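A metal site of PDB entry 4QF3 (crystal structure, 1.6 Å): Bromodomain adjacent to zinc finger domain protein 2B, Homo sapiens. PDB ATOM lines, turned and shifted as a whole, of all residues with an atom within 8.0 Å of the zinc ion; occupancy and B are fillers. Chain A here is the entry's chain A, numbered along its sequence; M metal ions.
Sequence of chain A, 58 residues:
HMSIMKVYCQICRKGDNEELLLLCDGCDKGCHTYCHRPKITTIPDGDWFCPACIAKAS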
ATOM      1  N   LEU A  23       5.983   8.502  16.431  1.00  0.00           N
ATOM      2  CA  LEU A  23       5.545   7.205  16.900  1.00  0.00           C
ATOM      3  C   LEU A  23       4.666   6.628  15.840  1.00  0.00           C
ATOM      4  O   LEU A  23       3.647   7.251  15.431  1.00  0.00           O
ATOM      5  CB  LEU A  23       4.769   7.314  18.223  1.00  0.00           C
ATOM      6  CG  LEU A  23       5.392   8.250  19.263  1.00  0.00           C
ATOM      7  CD1 LEU A  23       4.474   8.443  20.483  1.00  0.00           C
ATOM      8  CD2 LEU A  23       6.762   7.730  19.670  1.00  0.00           C
ATOM      9  N   CYS A  24       5.018   5.436  15.401  1.00  0.00           N
ATOM     10  CA  CYS A  24       4.347   4.763  14.290  1.00  0.00           C
ATOM     11  C   CYS A  24       3.021   4.170  14.751  1.00  0.00           C
ATOM     12  O   CYS A  24       2.998   3.389  15.687  1.00  0.00           O
ATOM     13  CB  CYS A  24       5.183   3.681  13.635  1.00  0.00           C
ATOM     14  SG  CYS A  24       4.345   2.894  12.220  1.00  0.00           S
ATOM     15  N   ASP A  25       1.961   4.499  14.021  1.00  0.00           N
ATOM     16  CA  ASP A  25       0.629   3.989  14.376  1.00  0.00           C
ATOM     17  C   ASP A  25       0.519   2.520  14.043  1.00  0.00           C
ATOM     18  O   ASP A  25      -0.324   1.804  14.605  1.00  0.00           O
ATOM     19  CB  ASP A  25      -0.462   4.735  13.625  1.00  0.00           C
ATOM     20  CG  ASP A  25      -1.180   5.710  14.478  1.00  0.00           C
ATOM     21  OD1 ASP A  25      -2.230   5.314  15.032  1.00  0.00           O
ATOM     22  OD2 ASP A  25      -0.674   6.833  14.606  1.00  0.00           O
ATOM     23  N   GLY A  26       1.353   2.067  13.104  1.00  0.00           N
ATOM     24  CA  GLY A  26       1.370   0.669  12.682  1.00  0.00           C
ATOM     25  C   GLY A  26       2.015  -0.270  13.680  1.00  0.00           C
ATOM     26  O   GLY A  26       1.386  -1.228  14.132  1.00  0.00           O
ATOM     27  N   CYS A  27       3.267   0.008  13.995  1.00  0.00           N
ATOM     28  CA  CYS A  27       4.121  -0.877  14.784  1.00  0.00           C
ATOM     29  C   CYS A  27       4.563  -0.347  16.150  1.00  0.00           C
ATOM     30  O   CYS A  27       5.272  -1.060  16.889  1.00  0.00           O
ATOM     31  CB  CYS A  27       5.393  -1.215  14.018  1.00  0.00           C
ATOM     32  SG  CYS A  27       6.502   0.198  13.739  1.00  0.00           S
ATOM     33  N   ASP A  28       4.163   0.870  16.476  1.00  0.00           N
ATOM     34  CA  ASP A  28       4.484   1.539  17.739  1.00  0.00           C
ATOM     35  C   ASP A  28       5.972   1.792  17.989  1.00  0.00           C
ATOM     36  O   ASP A  28       6.348   2.070  19.131  1.00  0.00           O
ATOM     37  CB  ASP A  28       3.882   0.766  18.937  1.00  0.00           C
ATOM     38  CG  ASP A  28       2.399   0.523  18.783  1.00  0.00           C
ATOM     39  OD1 ASP A  28       1.668   1.479  18.424  1.00  0.00           O
ATOM     40  OD2 ASP A  28       1.955  -0.612  19.049  1.00  0.00           O
ATOM     41  N   LYS A  29       6.818   1.731  16.948  1.00  0.00           N
ATOM     42  CA  LYS A  29       8.235   2.047  17.121  1.00  0.00           C
ATOM     43  C   LYS A  29       8.364   3.563  16.887  1.00  0.00           C
ATOM     44  O   LYS A  29       7.507   4.160  16.263  1.00  0.00           O
ATOM     45  CB  LYS A  29       9.062   1.317  16.149  1.00  0.00           C
ATOM     46  CG  LYS A  29       9.137  -0.186  16.455  1.00  0.00           C
ATOM     47  CD  LYS A  29       9.999  -0.905  15.457  1.00  0.00           C
ATOM     48  CE  LYS A  29      10.126  -2.365  15.884  1.00  0.00           C
ATOM     49  NZ  LYS A  29      10.599  -3.230  14.766  1.00  0.00           N
ATOM     50  N   GLY A  30       9.434   4.123  17.428  1.00  0.00           N
ATOM     51  CA  GLY A  30       9.715   5.564  17.416  1.00  0.00           C
ATOM     52  C   GLY A  30      10.975   5.925  16.676  1.00  0.00           C
ATOM     53  O   GLY A  30      11.925   5.153  16.576  1.00  0.00           O
ATOM     54  N   TRP A  48       1.405   9.118  12.148  1.00  0.00           N
ATOM     55  CA  TRP A  48       2.641   8.720  11.446  1.00  0.00           C
ATOM     56  C   TRP A  48       2.680   7.205  11.177  1.00  0.00           C
ATOM     57  O   TRP A  48       2.269   6.444  12.021  1.00  0.00           O
ATOM     58  CB  TRP A  48       3.813   9.126  12.329  1.00  0.00           C
ATOM     59  CG  TRP A  48       5.123   8.766  11.760  1.00  0.00           C
ATOM     60  CD1 TRP A  48       6.005   7.864  12.286  1.00  0.00           C
ATOM     61  CD2 TRP A  48       5.698   9.251  10.555  1.00  0.00           C
ATOM     62  NE1 TRP A  48       7.108   7.782  11.488  1.00  0.00           N
ATOM     63  CE2 TRP A  48       6.949   8.609  10.417  1.00  0.00           C
ATOM     64  CE3 TRP A  48       5.287  10.138   9.581  1.00  0.00           C
ATOM     65  CZ2 TRP A  48       7.802   8.868   9.359  1.00  0.00           C
ATOM     66  CZ3 TRP A  48       6.161  10.416   8.539  1.00  0.00           C
ATOM     67  CH2 TRP A  48       7.370   9.731   8.403  1.00  0.00           C
ATOM     68  N   PHE A  49       3.100   6.823   9.968  1.00  0.00           N
ATOM     69  CA  PHE A  49       3.448   5.429   9.641  1.00  0.00           C
ATOM     70  C   PHE A  49       4.874   5.438   9.162  1.00  0.00           C
ATOM     71  O   PHE A  49       5.243   6.230   8.241  1.00  0.00           O
ATOM     72  CB  PHE A  49       2.475   4.913   8.574  1.00  0.00           C
ATOM     73  CG  PHE A  49       1.080   4.726   9.118  1.00  0.00           C
ATOM     74  CD1 PHE A  49       0.761   3.576   9.819  1.00  0.00           C
ATOM     75  CD2 PHE A  49       0.124   5.731   8.953  1.00  0.00           C
ATOM     76  CE1 PHE A  49      -0.507   3.425  10.366  1.00  0.00           C
ATOM     77  CE2 PHE A  49      -1.151   5.567   9.498  1.00  0.00           C
ATOM     78  CZ  PHE A  49      -1.456   4.427  10.195  1.00  0.00           C
ATOM     79  N   CYS A  50       5.661   4.546   9.765  1.00  0.00           N
ATOM     80  CA  CYS A  50       7.109   4.557   9.564  1.00  0.00           C
ATOM     81  C   CYS A  50       7.447   3.938   8.217  1.00  0.00           C
ATOM     82  O   CYS A  50       6.652   3.277   7.560  1.00  0.00           O
ATOM     83  CB  CYS A  50       7.859   3.823  10.676  1.00  0.00           C
ATOM     84  SG  CYS A  50       7.739   2.033  10.560  1.00  0.00           S
ATOM     85  N   PRO A  51       8.683   4.165   7.744  1.00  0.00           N
ATOM     86  CA  PRO A  51       8.981   3.705   6.411  1.00  0.00           C
ATOM     87  C   PRO A  51       8.905   2.162   6.257  1.00  0.00           C
ATOM     88  O   PRO A  51       8.624   1.659   5.194  1.00  0.00           O
ATOM     89  CB  PRO A  51      10.423   4.229   6.208  1.00  0.00           C
ATOM     90  CG  PRO A  51      10.542   5.394   7.092  1.00  0.00           C
ATOM     91  CD  PRO A  51       9.737   5.035   8.295  1.00  0.00           C
ATOM     92  N   ALA A  52       9.195   1.441   7.341  1.00  0.00           N
ATOM     93  CA  ALA A  52       9.150  -0.031   7.273  1.00  0.00           C
ATOM     94  C   ALA A  52       7.701  -0.471   7.068  1.00  0.00           C
ATOM     95  O   ALA A  52       7.418  -1.338   6.249  1.00  0.00           O
ATOM     96  CB  ALA A  52       9.724  -0.650   8.530  1.00  0.00           C
ATOM     97  N   CYS A  53       6.783   0.173   7.797  1.00  0.00           N
ATOM     98  CA  CYS A  53       5.367  -0.171   7.636  1.00  0.00           C
ATOM     99  C   CYS A  53       4.801   0.209   6.283  1.00  0.00           C
ATOM    100  O   CYS A  53       4.099  -0.560   5.700  1.00  0.00           O
ATOM    101  CB  CYS A  53       4.532   0.443   8.743  1.00  0.00           C
ATOM    102  SG  CYS A  53       4.720  -0.347  10.370  1.00  0.00           S
ATOM    103  N   ILE A  54       5.202   1.354   5.741  1.00  0.00           N
ATOM    104  CA  ILE A  54       4.785   1.741   4.399  1.00  0.00           C
ATOM    105  C   ILE A  54       5.308   0.788   3.328  1.00  0.00           C
ATOM    106  O   ILE A  54       4.562   0.342   2.463  1.00  0.00           O
ATOM    107  CB  ILE A  54       5.226   3.207   4.165  1.00  0.00           C
ATOM    108  CG1 ILE A  54       4.507   4.170   5.116  1.00  0.00           C
ATOM    109  CG2 ILE A  54       4.938   3.610   2.728  1.00  0.00           C
ATOM    110  CD1 ILE A  54       2.981   4.209   4.985  1.00  0.00           C
ATOM    111  N   LYS A  56       6.035  -2.384   3.615  1.00  0.00           N
ATOM    112  CA  LYS A  56       5.307  -3.634   3.729  1.00  0.00           C
ATOM    113  C   LYS A  56       3.895  -3.525   3.207  1.00  0.00           C
ATOM    114  O   LYS A  56       3.417  -4.481   2.613  1.00  0.00           O
ATOM    115  CB  LYS A  56       5.193  -4.053   5.167  1.00  0.00           C
ATOM    116  CG  LYS A  56       6.399  -4.735   5.786  1.00  0.00           C
ATOM    117  CD  LYS A  56       6.000  -5.331   7.130  1.00  0.00           C
ATOM    118  CE  LYS A  56       7.211  -5.594   8.006  1.00  0.00           C
ATOM    119  NZ  LYS A  56       7.942  -4.343   8.341  1.00  0.00           N
HETATM  120 ZN    ZN M   1       5.858   1.192  11.721  1.00  0.00          ZN
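The side-chain sulfur (SG) of Cys 24 sits close to the backbone NH (N) of Gly 26 (3.2 Å).
The backbone NH (N) of Cys 24 sits at hydrogen-bond distance from the backbone carbonyl oxygen (O) of Lys 29 (2.9 Å).
SG of Cys 50 lies close to N of Ala 52 (3.6 Å).
The side-chain sulfur (SG) of Cys 27 lies close to the backbone NH (N) of Lys 29, at 3.6 Å.
The nearest printed residue that does not touch the zinc ion is Gly 26 (4.6 Å).
SG of Cys 24 binds the zinc ion (2.3 Å).
SG of Cys 27 is bound to the zinc ion (2.3 Å).
The zinc ion is bound by the side-chain sulfur (SG) of Cys 53, 2.3 Å away.
The side-chain sulfur (SG) of Cys 50 binds the zinc ion (2.4 Å).
The zinc ion has four donor atoms within binding distance.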
